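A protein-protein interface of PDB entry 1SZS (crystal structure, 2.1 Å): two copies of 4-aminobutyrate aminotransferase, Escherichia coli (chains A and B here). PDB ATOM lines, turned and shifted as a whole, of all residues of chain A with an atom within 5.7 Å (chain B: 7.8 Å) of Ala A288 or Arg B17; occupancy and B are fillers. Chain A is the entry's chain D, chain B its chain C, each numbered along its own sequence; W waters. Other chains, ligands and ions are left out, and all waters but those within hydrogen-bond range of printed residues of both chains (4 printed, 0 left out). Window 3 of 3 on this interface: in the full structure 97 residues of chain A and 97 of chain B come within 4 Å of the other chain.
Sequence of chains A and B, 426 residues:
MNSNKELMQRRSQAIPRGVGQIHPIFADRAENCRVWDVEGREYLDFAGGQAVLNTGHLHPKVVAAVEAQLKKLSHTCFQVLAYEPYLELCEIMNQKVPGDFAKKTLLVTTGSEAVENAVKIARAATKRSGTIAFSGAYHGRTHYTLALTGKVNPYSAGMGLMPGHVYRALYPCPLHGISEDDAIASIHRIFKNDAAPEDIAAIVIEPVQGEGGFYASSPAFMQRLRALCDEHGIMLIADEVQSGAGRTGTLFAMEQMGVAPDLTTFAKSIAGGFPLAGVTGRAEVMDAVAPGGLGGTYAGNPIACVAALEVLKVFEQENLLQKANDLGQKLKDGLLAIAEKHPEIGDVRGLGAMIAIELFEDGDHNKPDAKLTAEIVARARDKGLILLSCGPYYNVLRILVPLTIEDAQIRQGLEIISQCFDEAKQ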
ATOM      1  N   LYS A 104      -9.641 -30.578  -5.587  1.00  0.00           N
ATOM      2  CA  LYS A 104      -8.210 -30.817  -5.592  1.00  0.00           C
ATOM      3  C   LYS A 104      -7.583 -29.689  -4.748  1.00  0.00           C
ATOM      4  O   LYS A 104      -8.169 -28.602  -4.595  1.00  0.00           O
ATOM      5  CB  LYS A 104      -7.646 -30.839  -7.011  1.00  0.00           C
ATOM      6  CG  LYS A 104      -7.857 -32.172  -7.697  1.00  0.00           C
ATOM      7  CD  LYS A 104      -7.148 -32.213  -9.035  1.00  0.00           C
ATOM      8  CE  LYS A 104      -7.087 -33.617  -9.560  1.00  0.00           C
ATOM      9  NZ  LYS A 104      -6.054 -33.660 -10.649  1.00  0.00           N
ATOM     10  N   ILE A 121      -5.938 -19.590 -11.042  1.00  0.00           N
ATOM     11  CA  ILE A 121      -6.695 -20.774 -11.383  1.00  0.00           C
ATOM     12  C   ILE A 121      -8.099 -20.383 -11.917  1.00  0.00           C
ATOM     13  O   ILE A 121      -8.561 -20.981 -12.888  1.00  0.00           O
ATOM     14  CB  ILE A 121      -6.833 -21.707 -10.159  1.00  0.00           C
ATOM     15  CG1 ILE A 121      -5.487 -22.398  -9.896  1.00  0.00           C
ATOM     16  CG2 ILE A 121      -7.956 -22.716 -10.400  1.00  0.00           C
ATOM     17  CD1 ILE A 121      -5.295 -22.908  -8.479  1.00  0.00           C
ATOM     18  N   ALA A 124      -7.711 -19.171 -15.492  1.00  0.00           N
ATOM     19  CA  ALA A 124      -7.465 -20.240 -16.451  1.00  0.00           C
ATOM     20  C   ALA A 124      -8.746 -21.078 -16.703  1.00  0.00           C
ATOM     21  O   ALA A 124      -8.994 -21.521 -17.818  1.00  0.00           O
ATOM     22  CB  ALA A 124      -6.325 -21.131 -15.957  1.00  0.00           C
ATOM     23  N   ALA A 125      -9.555 -21.256 -15.668  1.00  0.00           N
ATOM     24  CA  ALA A 125     -10.773 -22.041 -15.775  1.00  0.00           C
ATOM     25  C   ALA A 125     -11.865 -21.330 -16.587  1.00  0.00           C
ATOM     26  O   ALA A 125     -12.545 -21.963 -17.387  1.00  0.00           O
ATOM     27  CB  ALA A 125     -11.306 -22.372 -14.371  1.00  0.00           C
ATOM     28  N   ALA A 283     -12.439 -29.562  -8.433  1.00  0.00           N
ATOM     29  CA  ALA A 283     -11.377 -30.219  -9.190  1.00  0.00           C
ATOM     30  C   ALA A 283     -11.136 -29.801 -10.643  1.00  0.00           C
ATOM     31  O   ALA A 283      -9.979 -29.534 -11.011  1.00  0.00           O
ATOM     32  CB  ALA A 283     -11.547 -31.765  -9.119  1.00  0.00           C
ATOM     33  N   GLU A 284     -12.187 -29.752 -11.466  1.00  0.00           N
ATOM     34  CA  GLU A 284     -12.002 -29.395 -12.868  1.00  0.00           C
ATOM     35  C   GLU A 284     -11.562 -27.930 -12.989  1.00  0.00           C
ATOM     36  O   GLU A 284     -10.914 -27.565 -13.970  1.00  0.00           O
ATOM     37  CB  GLU A 284     -13.276 -29.686 -13.709  1.00  0.00           C
ATOM     38  CG  GLU A 284     -14.541 -28.852 -13.411  1.00  0.00           C
ATOM     39  CD  GLU A 284     -15.274 -29.262 -12.149  1.00  0.00           C
ATOM     40  OE1 GLU A 284     -16.429 -28.809 -11.968  1.00  0.00           O
ATOM     41  OE2 GLU A 284     -14.718 -30.036 -11.329  1.00  0.00           O
ATOM     42  N   VAL A 285     -11.901 -27.102 -12.004  1.00  0.00           N
ATOM     43  CA  VAL A 285     -11.464 -25.707 -12.042  1.00  0.00           C
ATOM     44  C   VAL A 285      -9.943 -25.679 -11.717  1.00  0.00           C
ATOM     45  O   VAL A 285      -9.164 -25.091 -12.470  1.00  0.00           O
ATOM     46  CB  VAL A 285     -12.291 -24.853 -11.053  1.00  0.00           C
ATOM     47  CG1 VAL A 285     -11.666 -23.457 -10.877  1.00  0.00           C
ATOM     48  CG2 VAL A 285     -13.726 -24.720 -11.594  1.00  0.00           C
ATOM     49  N   MET A 286      -9.543 -26.364 -10.644  1.00  0.00           N
ATOM     50  CA  MET A 286      -8.132 -26.463 -10.252  1.00  0.00           C
ATOM     51  C   MET A 286      -7.309 -27.038 -11.397  1.00  0.00           C
ATOM     52  O   MET A 286      -6.189 -26.592 -11.639  1.00  0.00           O
ATOM     53  CB  MET A 286      -7.953 -27.407  -9.052  1.00  0.00           C
ATOM     54  CG  MET A 286      -8.697 -27.000  -7.795  1.00  0.00           C
ATOM     55  SD  MET A 286      -8.078 -25.462  -7.057  1.00  0.00           S
ATOM     56  CE  MET A 286      -6.623 -26.023  -6.347  1.00  0.00           C
ATOM     57  N   ASP A 287      -7.854 -28.030 -12.099  1.00  0.00           N
ATOM     58  CA  ASP A 287      -7.118 -28.664 -13.200  1.00  0.00           C
ATOM     59  C   ASP A 287      -7.137 -27.866 -14.504  1.00  0.00           C
ATOM     60  O   ASP A 287      -6.617 -28.335 -15.516  1.00  0.00           O
ATOM     61  CB  ASP A 287      -7.646 -30.102 -13.453  1.00  0.00           C
ATOM     62  CG  ASP A 287      -6.891 -31.164 -12.637  1.00  0.00           C
ATOM     63  OD1 ASP A 287      -7.407 -32.294 -12.494  1.00  0.00           O
ATOM     64  OD2 ASP A 287      -5.770 -30.878 -12.141  1.00  0.00           O
ATOM     65  N   ALA A 288      -7.726 -26.679 -14.495  1.00  0.00           N
ATOM     66  CA  ALA A 288      -7.758 -25.890 -15.726  1.00  0.00           C
ATOM     67  C   ALA A 288      -6.374 -25.398 -16.116  1.00  0.00           C
ATOM     68  O   ALA A 288      -6.154 -25.059 -17.277  1.00  0.00           O
ATOM     69  CB  ALA A 288      -8.715 -24.706 -15.577  1.00  0.00           C
ATOM     70  N   VAL A 289      -5.447 -25.361 -15.153  1.00  0.00           N
ATOM     71  CA  VAL A 289      -4.073 -24.909 -15.399  1.00  0.00           C
ATOM     72  C   VAL A 289      -3.183 -26.069 -15.869  1.00  0.00           C
ATOM     73  O   VAL A 289      -3.152 -27.116 -15.229  1.00  0.00           O
ATOM     74  CB  VAL A 289      -3.451 -24.280 -14.106  1.00  0.00           C
ATOM     75  CG1 VAL A 289      -1.990 -23.929 -14.332  1.00  0.00           C
ATOM     76  CG2 VAL A 289      -4.242 -23.036 -13.703  1.00  0.00           C
ATOM     77  N   ALA A 290      -2.463 -25.864 -16.971  1.00  0.00           N
ATOM     78  CA  ALA A 290      -1.570 -26.865 -17.559  1.00  0.00           C
ATOM     79  C   ALA A 290      -0.354 -27.173 -16.680  1.00  0.00           C
ATOM     80  O   ALA A 290       0.170 -26.279 -16.002  1.00  0.00           O
ATOM     81  CB  ALA A 290      -1.105 -26.377 -18.928  1.00  0.00           C
ATOM     82  N   PRO A 291       0.126 -28.439 -16.690  1.00  0.00           N
ATOM     83  CA  PRO A 291       1.283 -28.759 -15.851  1.00  0.00           C
ATOM     84  C   PRO A 291       2.421 -27.771 -15.972  1.00  0.00           C
ATOM     85  O   PRO A 291       2.726 -27.295 -17.064  1.00  0.00           O
ATOM     86  CB  PRO A 291       1.669 -30.183 -16.283  1.00  0.00           C
ATOM     87  CG  PRO A 291       0.674 -30.566 -17.345  1.00  0.00           C
ATOM     88  CD  PRO A 291      -0.485 -29.666 -17.227  1.00  0.00           C
ATOM     89  N   GLY A 292       3.043 -27.466 -14.837  1.00  0.00           N
ATOM     90  CA  GLY A 292       4.132 -26.511 -14.832  1.00  0.00           C
ATOM     91  C   GLY A 292       3.597 -25.130 -14.511  1.00  0.00           C
ATOM     92  O   GLY A 292       4.358 -24.197 -14.208  1.00  0.00           O
ATOM     93  N   ARG B  11      -1.913 -38.932  -6.161  1.00  0.00           N
ATOM     94  CA  ARG B  11      -1.586 -37.554  -6.481  1.00  0.00           C
ATOM     95  C   ARG B  11      -2.504 -37.031  -7.610  1.00  0.00           C
ATOM     96  O   ARG B  11      -3.077 -35.939  -7.478  1.00  0.00           O
ATOM     97  CB  ARG B  11      -0.108 -37.450  -6.912  1.00  0.00           C
ATOM     98  CG  ARG B  11       0.365 -36.036  -7.302  1.00  0.00           C
ATOM     99  CD  ARG B  11       1.473 -36.119  -8.340  1.00  0.00           C
ATOM    100  NE  ARG B  11       2.397 -34.979  -8.369  1.00  0.00           N
ATOM    101  CZ  ARG B  11       2.127 -33.771  -8.856  1.00  0.00           C
ATOM    102  NH1 ARG B  11       0.935 -33.476  -9.373  1.00  0.00           N
ATOM    103  NH2 ARG B  11       3.087 -32.863  -8.857  1.00  0.00           N
ATOM    104  N   SER B  12      -2.659 -37.818  -8.683  1.00  0.00           N
ATOM    105  CA  SER B  12      -3.491 -37.431  -9.835  1.00  0.00           C
ATOM    106  C   SER B  12      -4.903 -37.119  -9.425  1.00  0.00           C
ATOM    107  O   SER B  12      -5.593 -36.371 -10.112  1.00  0.00           O
ATOM    108  CB  SER B  12      -3.541 -38.550 -10.887  1.00  0.00           C
ATOM    109  OG  SER B  12      -4.388 -39.613 -10.454  1.00  0.00           O
ATOM    110  N   ALA B  14      -5.768 -36.017  -6.045  1.00  0.00           N
ATOM    111  CA  ALA B  14      -5.883 -35.017  -4.992  1.00  0.00           C
ATOM    112  C   ALA B  14      -5.266 -33.659  -5.293  1.00  0.00           C
ATOM    113  O   ALA B  14      -5.643 -32.647  -4.700  1.00  0.00           O
ATOM    114  CB  ALA B  14      -5.242 -35.561  -3.734  1.00  0.00           C
ATOM    115  N   ILE B  15      -4.333 -33.661  -6.226  1.00  0.00           N
ATOM    116  CA  ILE B  15      -3.535 -32.505  -6.531  1.00  0.00           C
ATOM    117  C   ILE B  15      -3.689 -32.084  -7.970  1.00  0.00           C
ATOM    118  O   ILE B  15      -3.737 -32.929  -8.865  1.00  0.00           O
ATOM    119  CB  ILE B  15      -2.061 -32.873  -6.205  1.00  0.00           C
ATOM    120  CG1 ILE B  15      -1.926 -33.117  -4.691  1.00  0.00           C
ATOM    121  CG2 ILE B  15      -1.098 -31.799  -6.675  1.00  0.00           C
ATOM    122  CD1 ILE B  15      -0.528 -33.616  -4.277  1.00  0.00           C
ATOM    123  N   PRO B  16      -3.750 -30.769  -8.221  1.00  0.00           N
ATOM    124  CA  PRO B  16      -3.906 -30.327  -9.605  1.00  0.00           C
ATOM    125  C   PRO B  16      -2.769 -30.707 -10.517  1.00  0.00           C
ATOM    126  O   PRO B  16      -1.603 -30.740 -10.110  1.00  0.00           O
ATOM    127  CB  PRO B  16      -4.077 -28.820  -9.481  1.00  0.00           C
ATOM    128  CG  PRO B  16      -3.409 -28.490  -8.187  1.00  0.00           C
ATOM    129  CD  PRO B  16      -3.798 -29.628  -7.293  1.00  0.00           C
ATOM    130  N   ARG B  17      -3.124 -30.995 -11.764  1.00  0.00           N
ATOM    131  CA  ARG B  17      -2.141 -31.360 -12.764  1.00  0.00           C
ATOM    132  C   ARG B  17      -1.199 -30.172 -13.049  1.00  0.00           C
ATOM    133  O   ARG B  17      -0.089 -30.369 -13.520  1.00  0.00           O
ATOM    134  CB  ARG B  17      -2.853 -31.789 -14.047  1.00  0.00           C
ATOM    135  CG  ARG B  17      -3.688 -30.697 -14.669  1.00  0.00           C
ATOM    136  CD  ARG B  17      -4.223 -31.046 -16.068  1.00  0.00           C
ATOM    137  NE  ARG B  17      -4.887 -29.855 -16.614  1.00  0.00           N
ATOM    138  CZ  ARG B  17      -4.613 -29.284 -17.788  1.00  0.00           C
ATOM    139  NH1 ARG B  17      -3.687 -29.791 -18.590  1.00  0.00           N
ATOM    140  NH2 ARG B  17      -5.242 -28.172 -18.139  1.00  0.00           N
ATOM    141  N   GLY B  18      -1.647 -28.950 -12.771  1.00  0.00           N
ATOM    142  CA  GLY B  18      -0.798 -27.789 -13.000  1.00  0.00           C
ATOM    143  C   GLY B  18       0.483 -27.837 -12.163  1.00  0.00           C
ATOM    144  O   GLY B  18       1.490 -27.216 -12.511  1.00  0.00           O
ATOM    145  N   VAL B  19       0.445 -28.553 -11.043  1.00  0.00           N
ATOM    146  CA  VAL B  19       1.639 -28.697 -10.213  1.00  0.00           C
ATOM    147  C   VAL B  19       2.443 -29.801 -10.934  1.00  0.00           C
ATOM    148  O   VAL B  19       2.109 -30.979 -10.833  1.00  0.00           O
ATOM    149  CB  VAL B  19       1.289 -29.161  -8.786  1.00  0.00           C
ATOM    150  CG1 VAL B  19       2.560 -29.325  -7.958  1.00  0.00           C
ATOM    151  CG2 VAL B  19       0.344 -28.163  -8.131  1.00  0.00           C
ATOM    152  N   GLY B  20       3.474 -29.409 -11.673  1.00  0.00           N
ATOM    153  CA  GLY B  20       4.277 -30.386 -12.404  1.00  0.00           C
ATOM    154  C   GLY B  20       5.042 -31.334 -11.496  1.00  0.00           C
ATOM    155  O   GLY B  20       5.125 -31.107 -10.301  1.00  0.00           O
ATOM    156  N   GLN B  21       5.579 -32.405 -12.065  1.00  0.00           N
ATOM    157  CA  GLN B  21       6.350 -33.397 -11.315  1.00  0.00           C
ATOM    158  C   GLN B  21       7.524 -33.852 -12.201  1.00  0.00           C
ATOM    159  O   GLN B  21       7.357 -34.690 -13.093  1.00  0.00           O
ATOM    160  CB  GLN B  21       5.458 -34.594 -10.962  1.00  0.00           C
ATOM    161  CG  GLN B  21       6.080 -35.559  -9.943  1.00  0.00           C
ATOM    162  CD  GLN B  21       6.176 -34.956  -8.561  1.00  0.00           C
ATOM    163  OE1 GLN B  21       5.162 -34.593  -7.966  1.00  0.00           O
ATOM    164  NE2 GLN B  21       7.397 -34.844  -8.037  1.00  0.00           N
ATOM    165  N   ALA B 157       0.717 -19.521 -18.641  1.00  0.00           N
ATOM    166  CA  ALA B 157      -0.037 -19.965 -19.811  1.00  0.00           C
ATOM    167  C   ALA B 157      -1.525 -20.152 -19.527  1.00  0.00           C
ATOM    168  O   ALA B 157      -1.890 -20.696 -18.484  1.00  0.00           O
ATOM    169  CB  ALA B 157       0.569 -21.271 -20.344  1.00  0.00           C
ATOM    170  N   GLY B 158      -2.367 -19.694 -20.455  1.00  0.00           N
ATOM    171  CA  GLY B 158      -3.811 -19.822 -20.327  1.00  0.00           C
ATOM    172  C   GLY B 158      -4.497 -18.935 -19.293  1.00  0.00           C
ATOM    173  O   GLY B 158      -5.713 -19.006 -19.109  1.00  0.00           O
ATOM    174  N   MET B 159      -3.743 -18.067 -18.637  1.00  0.00           N
ATOM    175  CA  MET B 159      -4.332 -17.222 -17.602  1.00  0.00           C
ATOM    176  C   MET B 159      -4.755 -15.830 -18.049  1.00  0.00           C
ATOM    177  O   MET B 159      -5.265 -15.065 -17.233  1.00  0.00           O
ATOM    178  CB  MET B 159      -3.345 -17.104 -16.442  1.00  0.00           C
ATOM    179  CG  MET B 159      -3.130 -18.397 -15.661  1.00  0.00           C
ATOM    180  SD  MET B 159      -1.617 -18.356 -14.692  1.00  0.00           S
ATOM    181  CE  MET B 159      -1.057 -20.122 -14.814  1.00  0.00           C
HETATM  182  O   HOH W   1      -2.458 -22.948 -17.798  1.00  0.00           O
HETATM  183  O   HOH W   2      -3.818 -27.458 -12.760  1.00  0.00           O
HETATM  184  O   HOH W   3      -7.202 -21.498 -19.832  1.00  0.00           O
HETATM  185  O   HOH W   4       4.619 -26.956 -11.832  1.00  0.00           O
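The guanidinium group (NH2) of Arg B17 is in hydrogen-bond range of the backbone carbonyl oxygen (O) of Ala A288 (3.4 Å).
The side-chain amino group of Lys A104 sits at hydrogen-bond distance from the backbone carbonyl oxygen of Ile B15.
The guanidinium group (NE) of Arg B17 sits at hydrogen-bond distance from the backbone carbonyl oxygen (O) of Asp A287 (2.6 Å).
The backbone NH of Gly A292 is in hydrogen-bond range of the backbone carbonyl oxygen of Gly B18 (2.8 Å).
The backbone carbonyl oxygen of Ser B12 sits at hydrogen-bond distance from the side-chain amino group of Lys A104, 2.8 Å away.
The backbone NH (N) of Gly B18 sits close to the backbone carbonyl oxygen (O) of Val A289 (3.4 Å).
NH2 of Arg B11 is in hydrogen-bond range of O of Gly B20 (3.1 Å).
NZ of Lys A104 is in salt-bridge range of OD1 of Asp A287 (2.7 Å).
Among the printed residues, merely in contact across the chains: Lys A104 with Ala B14, Lys A104 with Pro B16, Ala A124 with Gly B158, Met A286 with Pro B16, Asp A287 with Pro B16, Val A289 with Arg B17, Val A289 with Met B159, Ala A290 with Arg B17, Ala A290 with Gly B18, Pro A291 with Arg B17, Pro A291 with Gly B18 and Gly A292 with Gly B20.
Of the printed residues of chain B, Ala A124 touches Gly B158 (3.4 Å).
Of the printed residues of chain B, Met A286 touches Pro B16 (3.8 Å).
Ala A288 touches just one residue of chain B: Arg B17.
Arg B17 touches five residues of chain A.
The nearest residue of chain A that does not touch Arg B17 is Lys A104 (4.1 Å).
Hydrophobic or aromatic side chains of chain A that line the printed part of chain B: Ala A124, Val A289 and Pro A291.
Hydrophobic or aromatic side chains of chain B that line the printed part of chain A: Pro B16 and Met B159.
No position is printed for both chains.
Of the 18 pairs that touch across the chains among the printed residues, none has its exchanged pair printed and touching as well.
Water W1 lies within hydrogen-bond range of O of Ala B157 (2.4 Å) and N of Ala A290 (3.0 Å).
Water W2 lies within hydrogen-bond range of the backbone carbonyl oxygen (O) of Val A289 (2.6 Å), the backbone NH (N) of Gly B18 (2.6 Å) and the backbone carbonyl oxygen (O) of Met A286 (2.8 Å).
Water W3 bridges the backbone carbonyl oxygen (O) of Ala A124 (2.7 Å) and the backbone carbonyl oxygen (O) of Gly B158 (3.0 Å).
Water W4 lies within hydrogen-bond range of the backbone NH (N) of Gly B20 (2.7 Å), the backbone carbonyl oxygen (O) of Gly B18 (3.2 Å) and the backbone NH (N) of Gly A292 (3.4 Å).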
